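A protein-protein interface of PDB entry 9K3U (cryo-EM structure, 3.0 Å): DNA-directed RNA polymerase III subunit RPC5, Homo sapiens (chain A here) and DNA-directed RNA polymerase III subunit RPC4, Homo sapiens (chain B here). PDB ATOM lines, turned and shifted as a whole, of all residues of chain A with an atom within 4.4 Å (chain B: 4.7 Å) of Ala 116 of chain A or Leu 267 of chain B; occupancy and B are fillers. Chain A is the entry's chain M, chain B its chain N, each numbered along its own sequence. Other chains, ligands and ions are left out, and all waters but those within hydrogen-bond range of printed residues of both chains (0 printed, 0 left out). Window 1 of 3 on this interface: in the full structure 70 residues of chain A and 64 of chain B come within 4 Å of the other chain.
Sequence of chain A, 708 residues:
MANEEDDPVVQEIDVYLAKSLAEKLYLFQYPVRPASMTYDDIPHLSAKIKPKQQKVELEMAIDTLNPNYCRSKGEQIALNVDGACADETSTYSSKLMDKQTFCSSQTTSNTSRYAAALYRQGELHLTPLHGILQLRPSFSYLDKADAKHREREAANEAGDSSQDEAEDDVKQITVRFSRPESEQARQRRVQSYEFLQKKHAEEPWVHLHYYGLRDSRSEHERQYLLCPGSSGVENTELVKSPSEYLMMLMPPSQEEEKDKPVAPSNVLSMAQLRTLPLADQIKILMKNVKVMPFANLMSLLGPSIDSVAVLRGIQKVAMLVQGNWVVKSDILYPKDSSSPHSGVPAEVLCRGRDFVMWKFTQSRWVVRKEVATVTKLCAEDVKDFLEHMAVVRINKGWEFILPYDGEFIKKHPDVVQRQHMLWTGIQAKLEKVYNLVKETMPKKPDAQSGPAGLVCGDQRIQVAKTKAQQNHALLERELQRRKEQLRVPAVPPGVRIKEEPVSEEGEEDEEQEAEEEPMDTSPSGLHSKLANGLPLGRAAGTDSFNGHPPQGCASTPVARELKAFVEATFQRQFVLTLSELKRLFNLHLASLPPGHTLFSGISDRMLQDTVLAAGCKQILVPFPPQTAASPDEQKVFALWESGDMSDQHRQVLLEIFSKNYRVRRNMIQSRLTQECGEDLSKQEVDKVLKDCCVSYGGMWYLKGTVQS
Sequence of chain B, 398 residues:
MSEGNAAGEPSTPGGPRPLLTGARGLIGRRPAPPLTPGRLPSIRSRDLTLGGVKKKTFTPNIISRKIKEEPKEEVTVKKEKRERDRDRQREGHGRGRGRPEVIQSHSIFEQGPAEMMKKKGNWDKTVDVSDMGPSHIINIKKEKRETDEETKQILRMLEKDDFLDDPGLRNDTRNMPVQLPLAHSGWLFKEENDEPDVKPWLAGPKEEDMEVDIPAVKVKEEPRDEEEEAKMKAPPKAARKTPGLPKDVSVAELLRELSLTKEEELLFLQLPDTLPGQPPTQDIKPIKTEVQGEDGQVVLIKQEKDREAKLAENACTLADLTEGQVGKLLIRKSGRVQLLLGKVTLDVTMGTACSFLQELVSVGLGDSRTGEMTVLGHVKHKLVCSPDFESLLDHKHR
N of Ala 116 of chain A sits at hydrogen-bond distance from O of Thr 127 of chain A, 2.9 Å away.
The backbone NH (N) of Leu 118 of chain A sits at hydrogen-bond distance from the backbone carbonyl oxygen (O) of His 125 of chain A, at 2.9 Å.
The backbone NH of Leu 383 of chain B sits at hydrogen-bond distance from the backbone carbonyl oxygen of Phe 268 of chain B, at 2.9 Å.
Among the printed residues, merely in contact across the chains: Ala 117 of chain A with Leu 266 of chain B (3.6 Å), Leu 126 of chain A with Leu 269 of chain B (3.7 Å), Ala 116 of chain A with Leu 267 of chain B (3.7 Å), Leu 129 of chain A with Phe 268 of chain B (3.7 Å), Leu 25 of chain A with Leu 360 of chain B (3.7 Å), Ala 117 of chain A with Leu 269 of chain B (3.7 Å), Leu 118 of chain A with Leu 266 of chain B (3.8 Å), Ala 115 of chain A with Phe 268 of chain B (3.8 Å), Ala 116 of chain A with Leu 360 of chain B (3.9 Å) and Leu 118 of chain A with Glu 265 of chain B (3.99 Å).
Hydrophobic or aromatic side chains of chain B within 4 Å of the printed part of chain A: Leu 266, Leu 267, Phe 268, Leu 269 and Leu 360.
Of the 9 printed residues of chain A, 7 touch a printed residue of chain B.
Along chain A the printed residues that touch a printed residue of chain B span positions 25 to 129.
Among the printed residues, 12 pairs touch across the chains.
Among the printed residues, no Asp or Glu carboxylate lies within 4 Å of a Lys or Arg side-chain nitrogen of the other chain.
Of the printed residues of chain B, Ala 115 of chain A touches Phe 268 (3.8 Å) and Leu 269 (3.2 Å).
Ala 116 of chain A touches just these residues of chain B: Leu 267 and Leu 360.
Of the printed residues of chain B, Leu 126 of chain A touches Leu 269.
Of the printed residues of chain A, Glu 265 of chain B touches Leu 118.
Of the printed residues of chain A, Leu 266 of chain B touches Ala 117 and Leu 118.
Leu 267 of chain B touches just these residues of chain A: Ala 116 (3.7 Å) and Ala 117 (2.5 Å).
Of the printed residues of chain A, Leu 269 of chain B touches Ala 115, Ala 117 and Leu 126.
Leu 383 of chain B touches none of the printed residues of chain A.
The nearest printed residue of chain A that does not touch Phe 268 of chain B is Ala 117 of chain A (4.5 Å).
O of Ala 115 of chain A is in hydrogen-bond range of N of Leu 269 of chain B, at 3.4 Å.
The backbone NH (N) of Leu 267 of chain B lies within hydrogen-bond range of the backbone carbonyl oxygen (O) of Ala 117 of chain A (2.5 Å).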
ATOM      1  N   LEU A  25     -14.761   4.841 -19.074  1.00  0.00           N
ATOM      2  CA  LEU A  25     -13.773   3.799 -18.815  1.00  0.00           C
ATOM      3  C   LEU A  25     -14.490   2.494 -18.493  1.00  0.00           C
ATOM      4  O   LEU A  25     -15.249   2.421 -17.519  1.00  0.00           O
ATOM      5  CB  LEU A  25     -12.851   4.205 -17.664  1.00  0.00           C
ATOM      6  CG  LEU A  25     -11.697   3.246 -17.353  1.00  0.00           C
ATOM      7  CD1 LEU A  25     -10.737   3.156 -18.530  1.00  0.00           C
ATOM      8  CD2 LEU A  25     -10.964   3.686 -16.096  1.00  0.00           C
ATOM      9  N   ALA A 115     -11.413   1.065  -9.312  1.00  0.00           N
ATOM     10  CA  ALA A 115     -10.739   2.167  -9.981  1.00  0.00           C
ATOM     11  C   ALA A 115      -9.472   1.653 -10.644  1.00  0.00           C
ATOM     12  O   ALA A 115      -8.771   0.796 -10.099  1.00  0.00           O
ATOM     13  CB  ALA A 115     -10.402   3.296  -8.999  1.00  0.00           C
ATOM     14  N   ALA A 116      -9.183   2.189 -11.828  1.00  0.00           N
ATOM     15  CA  ALA A 116      -7.968   1.852 -12.553  1.00  0.00           C
ATOM     16  C   ALA A 116      -6.832   2.758 -12.098  1.00  0.00           C
ATOM     17  O   ALA A 116      -6.991   3.978 -12.004  1.00  0.00           O
ATOM     18  CB  ALA A 116      -8.178   1.993 -14.063  1.00  0.00           C
ATOM     19  N   ALA A 117      -5.681   2.149 -11.822  1.00  0.00           N
ATOM     20  CA  ALA A 117      -4.519   2.852 -11.297  1.00  0.00           C
ATOM     21  C   ALA A 117      -3.404   2.813 -12.331  1.00  0.00           C
ATOM     22  O   ALA A 117      -2.851   1.745 -12.611  1.00  0.00           O
ATOM     23  CB  ALA A 117      -4.054   2.233  -9.977  1.00  0.00           C
ATOM     24  N   LEU A 118      -3.078   3.973 -12.893  1.00  0.00           N
ATOM     25  CA  LEU A 118      -1.975   4.116 -13.833  1.00  0.00           C
ATOM     26  C   LEU A 118      -0.756   4.612 -13.066  1.00  0.00           C
ATOM     27  O   LEU A 118      -0.813   5.655 -12.407  1.00  0.00           O
ATOM     28  CB  LEU A 118      -2.342   5.079 -14.963  1.00  0.00           C
ATOM     29  CG  LEU A 118      -1.336   5.206 -16.112  1.00  0.00           C
ATOM     30  CD1 LEU A 118      -2.048   5.618 -17.392  1.00  0.00           C
ATOM     31  CD2 LEU A 118      -0.233   6.202 -15.781  1.00  0.00           C
ATOM     32  N   HIS A 125      -2.091   7.566 -10.622  1.00  0.00           N
ATOM     33  CA  HIS A 125      -3.335   8.230 -10.992  1.00  0.00           C
ATOM     34  C   HIS A 125      -4.487   7.235 -10.949  1.00  0.00           C
ATOM     35  O   HIS A 125      -4.408   6.162 -11.556  1.00  0.00           O
ATOM     36  CB  HIS A 125      -3.223   8.844 -12.389  1.00  0.00           C
ATOM     37  CG  HIS A 125      -2.172   9.907 -12.498  1.00  0.00           C
ATOM     38  ND1 HIS A 125      -2.478  11.242 -12.637  1.00  0.00           N
ATOM     39  CD2 HIS A 125      -0.821   9.830 -12.484  1.00  0.00           C
ATOM     40  CE1 HIS A 125      -1.359  11.943 -12.708  1.00  0.00           C
ATOM     41  NE2 HIS A 125      -0.340  11.109 -12.616  1.00  0.00           N
ATOM     42  N   LEU A 126      -5.552   7.598 -10.241  1.00  0.00           N
ATOM     43  CA  LEU A 126      -6.725   6.751 -10.091  1.00  0.00           C
ATOM     44  C   LEU A 126      -7.882   7.312 -10.908  1.00  0.00           C
ATOM     45  O   LEU A 126      -8.207   8.499 -10.812  1.00  0.00           O
ATOM     46  CB  LEU A 126      -7.133   6.643  -8.622  1.00  0.00           C
ATOM     47  CG  LEU A 126      -6.004   6.319  -7.641  1.00  0.00           C
ATOM     48  CD1 LEU A 126      -6.551   6.159  -6.229  1.00  0.00           C
ATOM     49  CD2 LEU A 126      -5.248   5.073  -8.072  1.00  0.00           C
ATOM     50  N   THR A 127      -8.505   6.443 -11.707  1.00  0.00           N
ATOM     51  CA  THR A 127      -9.632   6.818 -12.551  1.00  0.00           C
ATOM     52  C   THR A 127     -10.791   5.871 -12.265  1.00  0.00           C
ATOM     53  O   THR A 127     -10.620   4.642 -12.356  1.00  0.00           O
ATOM     54  CB  THR A 127      -9.250   6.763 -14.036  1.00  0.00           C
ATOM     55  OG1 THR A 127      -8.123   7.616 -14.278  1.00  0.00           O
ATOM     56  CG2 THR A 127     -10.416   7.210 -14.906  1.00  0.00           C
ATOM     57  N   LEU A 129     -14.145   3.563 -12.683  1.00  0.00           N
ATOM     58  CA  LEU A 129     -14.644   2.697 -13.742  1.00  0.00           C
ATOM     59  C   LEU A 129     -16.157   2.827 -13.831  1.00  0.00           C
ATOM     60  O   LEU A 129     -16.848   2.808 -12.807  1.00  0.00           O
ATOM     61  CB  LEU A 129     -14.263   1.235 -13.493  1.00  0.00           C
ATOM     62  CG  LEU A 129     -12.900   0.785 -14.019  1.00  0.00           C
ATOM     63  CD1 LEU A 129     -11.775   1.486 -13.286  1.00  0.00           C
ATOM     64  CD2 LEU A 129     -12.760  -0.724 -13.898  1.00  0.00           C
ATOM     65  N   GLU B 257       9.286  -2.192  -9.962  1.00  0.00           N
ATOM     66  CA  GLU B 257       8.670  -1.385 -11.008  1.00  0.00           C
ATOM     67  C   GLU B 257       9.292   0.000 -11.106  1.00  0.00           C
ATOM     68  O   GLU B 257       9.337   0.576 -12.201  1.00  0.00           O
ATOM     69  CB  GLU B 257       7.165  -1.260 -10.759  1.00  0.00           C
ATOM     70  CG  GLU B 257       6.377  -2.522 -11.076  1.00  0.00           C
ATOM     71  CD  GLU B 257       4.908  -2.391 -10.727  1.00  0.00           C
ATOM     72  OE1 GLU B 257       4.508  -1.324 -10.215  1.00  0.00           O
ATOM     73  OE2 GLU B 257       4.150  -3.355 -10.967  1.00  0.00           O
ATOM     74  N   GLU B 265       3.250   1.140 -15.719  1.00  0.00           N
ATOM     75  CA  GLU B 265       2.457  -0.073 -15.594  1.00  0.00           C
ATOM     76  C   GLU B 265       1.043   0.291 -15.167  1.00  0.00           C
ATOM     77  O   GLU B 265       0.846   1.191 -14.347  1.00  0.00           O
ATOM     78  CB  GLU B 265       3.080  -1.040 -14.573  1.00  0.00           C
ATOM     79  CG  GLU B 265       2.326  -2.353 -14.406  1.00  0.00           C
ATOM     80  CD  GLU B 265       2.323  -3.191 -15.671  1.00  0.00           C
ATOM     81  OE1 GLU B 265       3.082  -2.864 -16.606  1.00  0.00           O
ATOM     82  OE2 GLU B 265       1.558  -4.178 -15.728  1.00  0.00           O
ATOM     83  N   LEU B 266       0.066  -0.414 -15.732  1.00  0.00           N
ATOM     84  CA  LEU B 266      -1.336  -0.213 -15.393  1.00  0.00           C
ATOM     85  C   LEU B 266      -1.722  -1.181 -14.278  1.00  0.00           C
ATOM     86  O   LEU B 266      -1.586  -2.400 -14.435  1.00  0.00           O
ATOM     87  CB  LEU B 266      -2.229  -0.419 -16.614  1.00  0.00           C
ATOM     88  CG  LEU B 266      -2.337   0.743 -17.606  1.00  0.00           C
ATOM     89  CD1 LEU B 266      -3.017   1.942 -16.959  1.00  0.00           C
ATOM     90  CD2 LEU B 266      -0.972   1.127 -18.152  1.00  0.00           C
ATOM     91  N   LEU B 267      -2.199  -0.638 -13.163  1.00  0.00           N
ATOM     92  CA  LEU B 267      -2.622  -1.427 -12.020  1.00  0.00           C
ATOM     93  C   LEU B 267      -4.119  -1.256 -11.798  1.00  0.00           C
ATOM     94  O   LEU B 267      -4.728  -0.277 -12.240  1.00  0.00           O
ATOM     95  CB  LEU B 267      -1.858  -1.024 -10.751  1.00  0.00           C
ATOM     96  CG  LEU B 267      -0.337  -1.171 -10.807  1.00  0.00           C
ATOM     97  CD1 LEU B 267       0.294  -0.669  -9.515  1.00  0.00           C
ATOM     98  CD2 LEU B 267       0.060  -2.615 -11.071  1.00  0.00           C
ATOM     99  N   PHE B 268      -4.709  -2.230 -11.106  1.00  0.00           N
ATOM    100  CA  PHE B 268      -6.133  -2.227 -10.778  1.00  0.00           C
ATOM    101  C   PHE B 268      -6.256  -2.469  -9.277  1.00  0.00           C
ATOM    102  O   PHE B 268      -5.935  -3.557  -8.790  1.00  0.00           O
ATOM    103  CB  PHE B 268      -6.885  -3.284 -11.579  1.00  0.00           C
ATOM    104  CG  PHE B 268      -8.347  -3.373 -11.242  1.00  0.00           C
ATOM    105  CD1 PHE B 268      -9.262  -2.524 -11.843  1.00  0.00           C
ATOM    106  CD2 PHE B 268      -8.806  -4.307 -10.329  1.00  0.00           C
ATOM    107  CE1 PHE B 268     -10.607  -2.605 -11.537  1.00  0.00           C
ATOM    108  CE2 PHE B 268     -10.150  -4.393 -10.019  1.00  0.00           C
ATOM    109  CZ  PHE B 268     -11.052  -3.540 -10.623  1.00  0.00           C
ATOM    110  N   LEU B 269      -6.705  -1.454  -8.547  1.00  0.00           N
ATOM    111  CA  LEU B 269      -6.852  -1.541  -7.103  1.00  0.00           C
ATOM    112  C   LEU B 269      -8.320  -1.444  -6.705  1.00  0.00           C
ATOM    113  O   LEU B 269      -9.093  -0.671  -7.276  1.00  0.00           O
ATOM    114  CB  LEU B 269      -6.039  -0.447  -6.404  1.00  0.00           C
ATOM    115  CG  LEU B 269      -6.097   0.979  -6.960  1.00  0.00           C
ATOM    116  CD1 LEU B 269      -7.441   1.639  -6.688  1.00  0.00           C
ATOM    117  CD2 LEU B 269      -4.962   1.806  -6.377  1.00  0.00           C
ATOM    118  N   LEU B 360      -7.583  -3.009 -20.539  1.00  0.00           N
ATOM    119  CA  LEU B 360      -8.246  -1.789 -20.089  1.00  0.00           C
ATOM    120  C   LEU B 360      -8.567  -0.933 -21.306  1.00  0.00           C
ATOM    121  O   LEU B 360      -7.679  -0.614 -22.103  1.00  0.00           O
ATOM    122  CB  LEU B 360      -7.357  -1.035 -19.101  1.00  0.00           C
ATOM    123  CG  LEU B 360      -7.961   0.228 -18.478  1.00  0.00           C
ATOM    124  CD1 LEU B 360      -9.188  -0.112 -17.649  1.00  0.00           C
ATOM    125  CD2 LEU B 360      -6.923   0.954 -17.634  1.00  0.00           C
ATOM    126  N   HIS B 381      -1.503  -6.990 -12.604  1.00  0.00           N
ATOM    127  CA  HIS B 381      -1.554  -7.168 -11.160  1.00  0.00           C
ATOM    128  C   HIS B 381      -2.820  -6.539 -10.595  1.00  0.00           C
ATOM    129  O   HIS B 381      -3.418  -5.647 -11.204  1.00  0.00           O
ATOM    130  CB  HIS B 381      -0.324  -6.551 -10.491  1.00  0.00           C
ATOM    131  CG  HIS B 381       0.975  -7.124 -10.962  1.00  0.00           C
ATOM    132  ND1 HIS B 381       1.445  -6.950 -12.246  1.00  0.00           N
ATOM    133  CD2 HIS B 381       1.904  -7.872 -10.323  1.00  0.00           C
ATOM    134  CE1 HIS B 381       2.607  -7.562 -12.378  1.00  0.00           C
ATOM    135  NE2 HIS B 381       2.907  -8.132 -11.225  1.00  0.00           N
ATOM    136  N   LEU B 383      -4.543  -5.108  -6.767  1.00  0.00           N
ATOM    137  CA  LEU B 383      -4.317  -4.693  -5.390  1.00  0.00           C
ATOM    138  C   LEU B 383      -5.648  -4.502  -4.676  1.00  0.00           C
ATOM    139  O   LEU B 383      -6.686  -4.277  -5.300  1.00  0.00           O
ATOM    140  CB  LEU B 383      -3.507  -3.391  -5.337  1.00  0.00           C
ATOM    141  CG  LEU B 383      -2.176  -3.388  -6.092  1.00  0.00           C
ATOM    142  CD1 LEU B 383      -1.539  -2.009  -6.039  1.00  0.00           C
ATOM    143  CD2 LEU B 383      -1.230  -4.438  -5.531  1.00  0.00           C
